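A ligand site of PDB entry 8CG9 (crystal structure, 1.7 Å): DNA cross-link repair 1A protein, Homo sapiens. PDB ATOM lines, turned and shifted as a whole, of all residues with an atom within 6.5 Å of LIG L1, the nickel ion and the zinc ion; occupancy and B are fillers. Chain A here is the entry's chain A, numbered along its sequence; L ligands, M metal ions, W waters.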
ATOM      1  N   HIS A  37      10.426  15.678 -34.027  1.00  0.00           N
ATOM      2  CA  HIS A  37      11.085  16.691 -34.840  1.00  0.00           C
ATOM      3  C   HIS A  37      12.296  16.092 -35.537  1.00  0.00           C
ATOM      4  O   HIS A  37      12.774  15.017 -35.181  1.00  0.00           O
ATOM      5  CB  HIS A  37      11.482  17.901 -33.986  1.00  0.00           C
ATOM      6  CG  HIS A  37      12.532  17.630 -32.960  1.00  0.00           C
ATOM      7  ND1 HIS A  37      12.340  16.796 -31.878  1.00  0.00           N
ATOM      8  CD2 HIS A  37      13.783  18.133 -32.825  1.00  0.00           C
ATOM      9  CE1 HIS A  37      13.431  16.781 -31.131  1.00  0.00           C
ATOM     10  NE2 HIS A  37      14.319  17.594 -31.683  1.00  0.00           N
ATOM     11  N   PHE A  38      12.797  16.826 -36.537  1.00  0.00           N
ATOM     12  CA  PHE A  38      13.858  16.316 -37.398  1.00  0.00           C
ATOM     13  C   PHE A  38      15.231  16.737 -36.860  1.00  0.00           C
ATOM     14  O   PHE A  38      15.965  17.543 -37.429  1.00  0.00           O
ATOM     15  CB  PHE A  38      13.642  16.806 -38.828  1.00  0.00           C
ATOM     16  CG  PHE A  38      14.528  16.121 -39.835  1.00  0.00           C
ATOM     17  CD1 PHE A  38      14.301  14.816 -40.200  1.00  0.00           C
ATOM     18  CD2 PHE A  38      15.590  16.808 -40.421  1.00  0.00           C
ATOM     19  CE1 PHE A  38      15.105  14.182 -41.134  1.00  0.00           C
ATOM     20  CE2 PHE A  38      16.400  16.181 -41.345  1.00  0.00           C
ATOM     21  CZ  PHE A  38      16.164  14.868 -41.701  1.00  0.00           C
ATOM     22  N   HIS A  39      15.560  16.153 -35.702  1.00  0.00           N
ATOM     23  CA  HIS A  39      16.884  16.259 -35.107  1.00  0.00           C
ATOM     24  C   HIS A  39      17.486  14.868 -34.968  1.00  0.00           C
ATOM     25  O   HIS A  39      16.785  13.913 -34.621  1.00  0.00           O
ATOM     26  CB  HIS A  39      16.834  16.940 -33.744  1.00  0.00           C
ATOM     27  CG  HIS A  39      16.925  18.426 -33.823  1.00  0.00           C
ATOM     28  ND1 HIS A  39      16.680  19.253 -32.739  1.00  0.00           N
ATOM     29  CD2 HIS A  39      17.240  19.251 -34.851  1.00  0.00           C
ATOM     30  CE1 HIS A  39      16.835  20.515 -33.099  1.00  0.00           C
ATOM     31  NE2 HIS A  39      17.171  20.539 -34.379  1.00  0.00           N
ATOM     32  N   ASP A  41      19.483  13.105 -33.032  1.00  0.00           N
ATOM     33  CA  ASP A  41      19.362  12.272 -31.831  1.00  0.00           C
ATOM     34  C   ASP A  41      17.990  11.630 -31.722  1.00  0.00           C
ATOM     35  O   ASP A  41      17.835  10.622 -31.023  1.00  0.00           O
ATOM     36  CB  ASP A  41      19.646  13.127 -30.587  1.00  0.00           C
ATOM     37  CG  ASP A  41      19.928  12.277 -29.352  1.00  0.00           C
ATOM     38  OD1 ASP A  41      20.981  11.604 -29.323  1.00  0.00           O
ATOM     39  OD2 ASP A  41      19.107  12.301 -28.406  1.00  0.00           O
ATOM     40  N   HIS A  42      16.994  12.152 -32.443  1.00  0.00           N
ATOM     41  CA  HIS A  42      15.618  11.701 -32.319  1.00  0.00           C
ATOM     42  C   HIS A  42      15.120  10.869 -33.496  1.00  0.00           C
ATOM     43  O   HIS A  42      14.325   9.948 -33.289  1.00  0.00           O
ATOM     44  CB  HIS A  42      14.699  12.913 -32.106  1.00  0.00           C
ATOM     45  CG  HIS A  42      15.074  13.731 -30.903  1.00  0.00           C
ATOM     46  ND1 HIS A  42      14.379  13.664 -29.714  1.00  0.00           N
ATOM     47  CD2 HIS A  42      16.088  14.603 -30.703  1.00  0.00           C
ATOM     48  CE1 HIS A  42      14.948  14.471 -28.832  1.00  0.00           C
ATOM     49  NE2 HIS A  42      15.992  15.051 -29.413  1.00  0.00           N
ATOM     50  N   HIS A  98      10.614  24.691 -30.538  1.00  0.00           N
ATOM     51  CA  HIS A  98      11.946  24.105 -30.616  1.00  0.00           C
ATOM     52  C   HIS A  98      12.482  24.488 -31.975  1.00  0.00           C
ATOM     53  O   HIS A  98      12.830  25.663 -32.184  1.00  0.00           O
ATOM     54  CB  HIS A  98      11.850  22.586 -30.358  1.00  0.00           C
ATOM     55  CG  HIS A  98      13.172  21.883 -30.310  1.00  0.00           C
ATOM     56  ND1 HIS A  98      14.218  22.312 -29.526  1.00  0.00           N
ATOM     57  CD2 HIS A  98      13.608  20.772 -30.947  1.00  0.00           C
ATOM     58  CE1 HIS A  98      15.240  21.486 -29.667  1.00  0.00           C
ATOM     59  NE2 HIS A  98      14.895  20.540 -30.517  1.00  0.00           N
ATOM     60  N   CYS A  99      12.567  23.586 -32.927  1.00  0.00           N
ATOM     61  CA  CYS A  99      12.986  23.886 -34.291  1.00  0.00           C
ATOM     62  C   CYS A  99      11.785  23.793 -35.224  1.00  0.00           C
ATOM     63  O   CYS A  99      10.696  23.385 -34.814  1.00  0.00           O
ATOM     64  CB  CYS A  99      14.083  22.892 -34.709  1.00  0.00           C
ATOM     65  SG  CYS A  99      13.476  21.215 -34.785  1.00  0.00           S
ATOM     66  N   ASP A 120      11.310  17.615 -27.782  1.00  0.00           N
ATOM     67  CA  ASP A 120      12.167  18.723 -27.362  1.00  0.00           C
ATOM     68  C   ASP A 120      11.348  20.002 -27.428  1.00  0.00           C
ATOM     69  O   ASP A 120      10.652  20.247 -28.425  1.00  0.00           O
ATOM     70  CB  ASP A 120      13.378  18.858 -28.290  1.00  0.00           C
ATOM     71  CG  ASP A 120      14.500  17.906 -27.949  1.00  0.00           C
ATOM     72  OD1 ASP A 120      14.412  17.177 -26.943  1.00  0.00           O
ATOM     73  OD2 ASP A 120      15.490  17.921 -28.703  1.00  0.00           O
ATOM     74  N   ASP A 143      11.032  16.986 -21.640  1.00  0.00           N
ATOM     75  CA  ASP A 143      12.360  17.385 -22.073  1.00  0.00           C
ATOM     76  C   ASP A 143      13.112  18.045 -20.923  1.00  0.00           C
ATOM     77  O   ASP A 143      12.911  19.233 -20.630  1.00  0.00           O
ATOM     78  CB  ASP A 143      12.262  18.335 -23.276  1.00  0.00           C
ATOM     79  CG  ASP A 143      13.607  18.933 -23.691  1.00  0.00           C
ATOM     80  OD1 ASP A 143      14.662  18.469 -23.203  1.00  0.00           O
ATOM     81  OD2 ASP A 143      13.601  19.872 -24.511  1.00  0.00           O
ATOM     82  N   THR A 145      16.421  18.628 -20.625  1.00  0.00           N
ATOM     83  CA  THR A 145      17.786  18.936 -21.037  1.00  0.00           C
ATOM     84  C   THR A 145      18.515  19.811 -20.024  1.00  0.00           C
ATOM     85  O   THR A 145      19.643  19.508 -19.614  1.00  0.00           O
ATOM     86  CB  THR A 145      17.777  19.612 -22.418  1.00  0.00           C
ATOM     87  OG1 THR A 145      17.310  18.685 -23.393  1.00  0.00           O
ATOM     88  CG2 THR A 145      19.159  20.090 -22.793  1.00  0.00           C
ATOM     89  N   TYR A 146      17.892  20.905 -19.610  1.00  0.00           N
ATOM     90  CA  TYR A 146      18.508  21.884 -18.718  1.00  0.00           C
ATOM     91  C   TYR A 146      17.839  21.905 -17.353  1.00  0.00           C
ATOM     92  O   TYR A 146      17.645  22.965 -16.750  1.00  0.00           O
ATOM     93  CB  TYR A 146      18.483  23.264 -19.356  1.00  0.00           C
ATOM     94  CG  TYR A 146      19.352  23.355 -20.584  1.00  0.00           C
ATOM     95  CD1 TYR A 146      20.713  23.127 -20.498  1.00  0.00           C
ATOM     96  CD2 TYR A 146      18.812  23.641 -21.835  1.00  0.00           C
ATOM     97  CE1 TYR A 146      21.514  23.198 -21.614  1.00  0.00           C
ATOM     98  CE2 TYR A 146      19.613  23.713 -22.961  1.00  0.00           C
ATOM     99  CZ  TYR A 146      20.965  23.477 -22.846  1.00  0.00           C
ATOM    100  OH  TYR A 146      21.779  23.549 -23.960  1.00  0.00           O
ATOM    101  N   TYR A 151      21.258  26.521 -15.166  1.00  0.00           N
ATOM    102  CA  TYR A 151      20.967  26.752 -16.581  1.00  0.00           C
ATOM    103  C   TYR A 151      20.023  27.935 -16.704  1.00  0.00           C
ATOM    104  O   TYR A 151      18.799  27.805 -16.664  1.00  0.00           O
ATOM    105  CB  TYR A 151      20.399  25.508 -17.234  1.00  0.00           C
ATOM    106  CG  TYR A 151      21.421  24.405 -17.322  1.00  0.00           C
ATOM    107  CD1 TYR A 151      22.580  24.591 -18.072  1.00  0.00           C
ATOM    108  CD2 TYR A 151      21.230  23.205 -16.673  1.00  0.00           C
ATOM    109  CE1 TYR A 151      23.533  23.590 -18.165  1.00  0.00           C
ATOM    110  CE2 TYR A 151      22.176  22.197 -16.766  1.00  0.00           C
ATOM    111  CZ  TYR A 151      23.320  22.396 -17.508  1.00  0.00           C
ATOM    112  OH  TYR A 151      24.251  21.388 -17.593  1.00  0.00           O
ATOM    113  N   THR A 267      25.577  28.523 -29.452  1.00  0.00           N
ATOM    114  CA  THR A 267      25.653  27.469 -28.447  1.00  0.00           C
ATOM    115  C   THR A 267      24.621  27.692 -27.349  1.00  0.00           C
ATOM    116  O   THR A 267      24.432  28.819 -26.885  1.00  0.00           O
ATOM    117  CB  THR A 267      27.041  27.442 -27.798  1.00  0.00           C
ATOM    118  OG1 THR A 267      27.142  28.516 -26.861  1.00  0.00           O
ATOM    119  CG2 THR A 267      28.123  27.603 -28.860  1.00  0.00           C
ATOM    120  N   GLY A 268      23.953  26.617 -26.941  1.00  0.00           N
ATOM    121  CA  GLY A 268      23.044  26.711 -25.812  1.00  0.00           C
ATOM    122  C   GLY A 268      23.742  26.423 -24.504  1.00  0.00           C
ATOM    123  O   GLY A 268      24.156  25.283 -24.248  1.00  0.00           O
ATOM    124  N   TRP A 269      23.884  27.459 -23.663  1.00  0.00           N
ATOM    125  CA  TRP A 269      24.507  27.373 -22.337  1.00  0.00           C
ATOM    126  C   TRP A 269      25.992  27.070 -22.430  1.00  0.00           C
ATOM    127  O   TRP A 269      26.414  26.158 -23.154  1.00  0.00           O
ATOM    128  CB  TRP A 269      23.807  26.321 -21.469  1.00  0.00           C
ATOM    129  N   THR A 270      26.808  27.821 -21.703  1.00  0.00           N
ATOM    130  CA  THR A 270      28.256  27.593 -21.688  1.00  0.00           C
ATOM    131  C   THR A 270      28.779  27.436 -20.275  1.00  0.00           C
ATOM    132  O   THR A 270      28.739  28.372 -19.477  1.00  0.00           O
ATOM    133  CB  THR A 270      29.016  28.742 -22.375  1.00  0.00           C
ATOM    134  OG1 THR A 270      28.728  29.974 -21.708  1.00  0.00           O
ATOM    135  CG2 THR A 270      28.607  28.856 -23.837  1.00  0.00           C
ATOM    136  N   HIS A 299      15.874  24.954 -26.154  1.00  0.00           N
ATOM    137  CA  HIS A 299      15.368  24.181 -25.025  1.00  0.00           C
ATOM    138  C   HIS A 299      15.003  25.107 -23.872  1.00  0.00           C
ATOM    139  O   HIS A 299      15.504  26.227 -23.774  1.00  0.00           O
ATOM    140  CB  HIS A 299      16.387  23.163 -24.507  1.00  0.00           C
ATOM    141  CG  HIS A 299      16.701  22.038 -25.440  1.00  0.00           C
ATOM    142  ND1 HIS A 299      15.914  20.905 -25.530  1.00  0.00           N
ATOM    143  CD2 HIS A 299      17.757  21.824 -26.253  1.00  0.00           C
ATOM    144  CE1 HIS A 299      16.450  20.059 -26.400  1.00  0.00           C
ATOM    145  NE2 HIS A 299      17.567  20.597 -26.853  1.00  0.00           N
ATOM    146  N   VAL A 321      15.316  13.103 -20.997  1.00  0.00           N
ATOM    147  CA  VAL A 321      16.671  13.563 -21.255  1.00  0.00           C
ATOM    148  C   VAL A 321      17.491  13.452 -19.968  1.00  0.00           C
ATOM    149  O   VAL A 321      16.996  13.786 -18.877  1.00  0.00           O
ATOM    150  CB  VAL A 321      16.700  15.014 -21.774  1.00  0.00           C
ATOM    151  CG1 VAL A 321      18.143  15.430 -22.103  1.00  0.00           C
ATOM    152  CG2 VAL A 321      15.823  15.157 -23.016  1.00  0.00           C
ATOM    153  N   ASN A 322      18.744  13.012 -20.101  1.00  0.00           N
ATOM    154  CA  ASN A 322      19.663  12.860 -18.976  1.00  0.00           C
ATOM    155  C   ASN A 322      19.183  11.774 -18.024  1.00  0.00           C
ATOM    156  O   ASN A 322      19.333  11.873 -16.806  1.00  0.00           O
ATOM    157  CB  ASN A 322      19.881  14.177 -18.219  1.00  0.00           C
ATOM    158  CG  ASN A 322      20.396  15.277 -19.106  1.00  0.00           C
ATOM    159  OD1 ASN A 322      21.207  15.039 -20.009  1.00  0.00           O
ATOM    160  ND2 ASN A 322      19.928  16.495 -18.863  1.00  0.00           N
HETATM  161  C1  LIG L   1      25.341  22.390 -21.932  1.00  0.00           C
HETATM  162  C2  LIG L   1      26.073  22.712 -23.049  1.00  0.00           C
HETATM  163  C3  LIG L   1      25.686  22.248 -24.293  1.00  0.00           C
HETATM  164  C4  LIG L   1      24.560  21.439 -24.403  1.00  0.00           C
HETATM  165  C5  LIG L   1      23.812  21.130 -23.277  1.00  0.00           C
HETATM  166  C6  LIG L   1      24.213  21.595 -22.041  1.00  0.00           C
HETATM  167  O1  LIG L   1      22.682  20.335 -23.366  1.00  0.00           O
HETATM  168  C7  LIG L   1      22.170  20.214 -24.706  1.00  0.00           C
HETATM  169  C8  LIG L   1      23.277  19.921 -25.677  1.00  0.00           C
HETATM  170  O2  LIG L   1      24.217  21.006 -25.662  1.00  0.00           O
HETATM  171  C9  LIG L   1      22.800  19.797 -27.134  1.00  0.00           C
HETATM  172  N1  LIG L   1      21.908  18.664 -27.427  1.00  0.00           N
HETATM  173  C10 LIG L   1      22.374  17.388 -27.633  1.00  0.00           C
HETATM  174  C11 LIG L   1      23.764  16.908 -27.581  1.00  0.00           C
HETATM  175  C12 LIG L   1      23.853  15.572 -27.830  1.00  0.00           C
HETATM  176  S1  LIG L   1      22.324  14.827 -28.124  1.00  0.00           S
HETATM  177  C13 LIG L   1      21.498  16.347 -27.912  1.00  0.00           C
HETATM  178  C14 LIG L   1      20.129  16.581 -27.998  1.00  0.00           C
HETATM  179  O3  LIG L   1      19.308  15.706 -28.257  1.00  0.00           O
HETATM  180  N2  LIG L   1      19.700  17.866 -27.799  1.00  0.00           N
HETATM  181  C15 LIG L   1      20.561  18.906 -27.511  1.00  0.00           C
HETATM  182  O4  LIG L   1      20.141  20.036 -27.335  1.00  0.00           O
HETATM  183  O5  LIG L   1      18.356  18.144 -27.871  1.00  0.00           O
HETATM  184  C1  LG2 L   2      27.053  18.474 -31.566  1.00  0.00           C
HETATM  185  C2  LG2 L   2      26.412  18.919 -30.427  1.00  0.00           C
HETATM  186  C3  LG2 L   2      25.171  18.413 -30.088  1.00  0.00           C
HETATM  187  C4  LG2 L   2      24.579  17.441 -30.887  1.00  0.00           C
HETATM  188  C5  LG2 L   2      25.221  16.995 -32.035  1.00  0.00           C
HETATM  189  C6  LG2 L   2      26.469  17.508 -32.374  1.00  0.00           C
HETATM  190  O1  LG2 L   2      24.666  16.032 -32.850  1.00  0.00           O
HETATM  191  C7  LG2 L   2      23.678  15.240 -32.178  1.00  0.00           C
HETATM  192  C8  LG2 L   2      22.678  16.102 -31.430  1.00  0.00           C
HETATM  193  O2  LG2 L   2      23.346  16.963 -30.505  1.00  0.00           O
HETATM  194  C9  LG2 L   2      21.906  17.009 -32.397  1.00  0.00           C
HETATM  195  N1  LG2 L   2      20.841  17.778 -31.730  1.00  0.00           N
HETATM  196  C10 LG2 L   2      21.011  19.095 -31.361  1.00  0.00           C
HETATM  197  C11 LG2 L   2      22.207  19.941 -31.505  1.00  0.00           C
HETATM  198  C12 LG2 L   2      21.991  21.201 -31.040  1.00  0.00           C
HETATM  199  S1  LG2 L   2      20.422  21.437 -30.364  1.00  0.00           S
HETATM  200  C13 LG2 L   2      19.977  19.803 -30.753  1.00  0.00           C
HETATM  201  C14 LG2 L   2      18.752  19.187 -30.515  1.00  0.00           C
HETATM  202  O3  LG2 L   2      17.798  19.753 -29.992  1.00  0.00           O
HETATM  203  N2  LG2 L   2      18.620  17.880 -30.899  1.00  0.00           N
HETATM  204  C15 LG2 L   2      19.633  17.163 -31.511  1.00  0.00           C
HETATM  205  O4  LG2 L   2      19.481  16.002 -31.843  1.00  0.00           O
HETATM  206  O5  LG2 L   2      17.421  17.230 -30.690  1.00  0.00           O
HETATM  207 NI    NI M   1      15.992  18.744 -30.808  1.00  0.00          NI
HETATM  208 ZN    ZN M   2      17.178  16.520 -28.644  1.00  0.00          ZN
HETATM  209  O   HOH W   1      16.771  15.980 -26.671  1.00  0.00           O
HETATM  210  O   HOH W   2      18.806  17.111 -25.152  1.00  0.00           O
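An oxygen (O1) of LIG L1 sits close to the side-chain hydroxyl (OH) of Tyr 146 (3.4 Å).
O4 of LG2 L2 lies within hydrogen-bond range of N of Asp 41 (3.1 Å).
A ring nitrogen (NE2) of His 299 is in hydrogen-bond range of an oxygen (O4) of LIG L1 (2.7 Å).
An oxygen (O3) of LG2 L2 lies close to a ring nitrogen (NE2) of His 299 (3.3 Å).
NE2 of His 39 is in hydrogen-bond range of SG of Cys 99, at 3.8 Å.
O of Gly 268 is in hydrogen-bond range of OH of Tyr 146 (3.0 Å).
A ring nitrogen (ND1) of His 299 lies within hydrogen-bond range of the side-chain hydroxyl (OG1) of Thr 145.
OG1 of Thr 145 is in hydrogen-bond range of OD1 of Asp 143, 2.7 Å away.
The side-chain carboxylate of Asp 143 sits at hydrogen-bond distance from a ring nitrogen (ND1) of His 299 (2.7 Å).
The backbone carbonyl oxygen of Thr 145 lies within hydrogen-bond range of the side-chain amide nitrogen of Asn 322 (3.1 Å).
The zinc ion is bound by NE2 of His 42 (2.0 Å).
Water W1 is bound to the zinc ion (2.1 Å).
The zinc ion is bound by O5 of LIG L1 (2.2 Å).
O5 of LG2 L2 binds the zinc ion, 2.2 Å away.
OD2 of Asp 120 binds the zinc ion (2.2 Å).
The zinc ion is bound by an oxygen (O3) of LIG L1 (2.3 Å).
Of the 19 residues printed, 2 come within 4 Å of the zinc ion.
Along chain A the residues within 4 Å of the zinc ion span positions 42 to 120.
The nickel ion is bound by O5 of LG2 L2 (2.1 Å), ND1 of His 39 (2.1 Å), NE2 of His 98 (2.1 Å), NE2 of His 37 (2.2 Å), O3 of LG2 L2 (2.2 Å) and OD2 of Asp 120 (2.3 Å).
Five residues have an atom within 4 Å of the nickel ion: His 37, His 39, His 42, His 98 and Asp 120.
An oxygen (O3) of LIG L1 lies close to the side-chain carboxylate (OD2) of Asp 41, at 3.4 Å.
Merely in contact with LIG L1: Gly 268 (3.4 Å), Trp 269 (3.5 Å) and Thr 145 (3.6 Å).
Eight residues have an atom within 4 Å of LIG L1: Asp 41, His 42, Asp 120, Thr 145, Tyr 146, Gly 268, Trp 269 and His 299.
The nearest printed residue that does not touch LIG L1 is Tyr 151 (4.3 Å).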
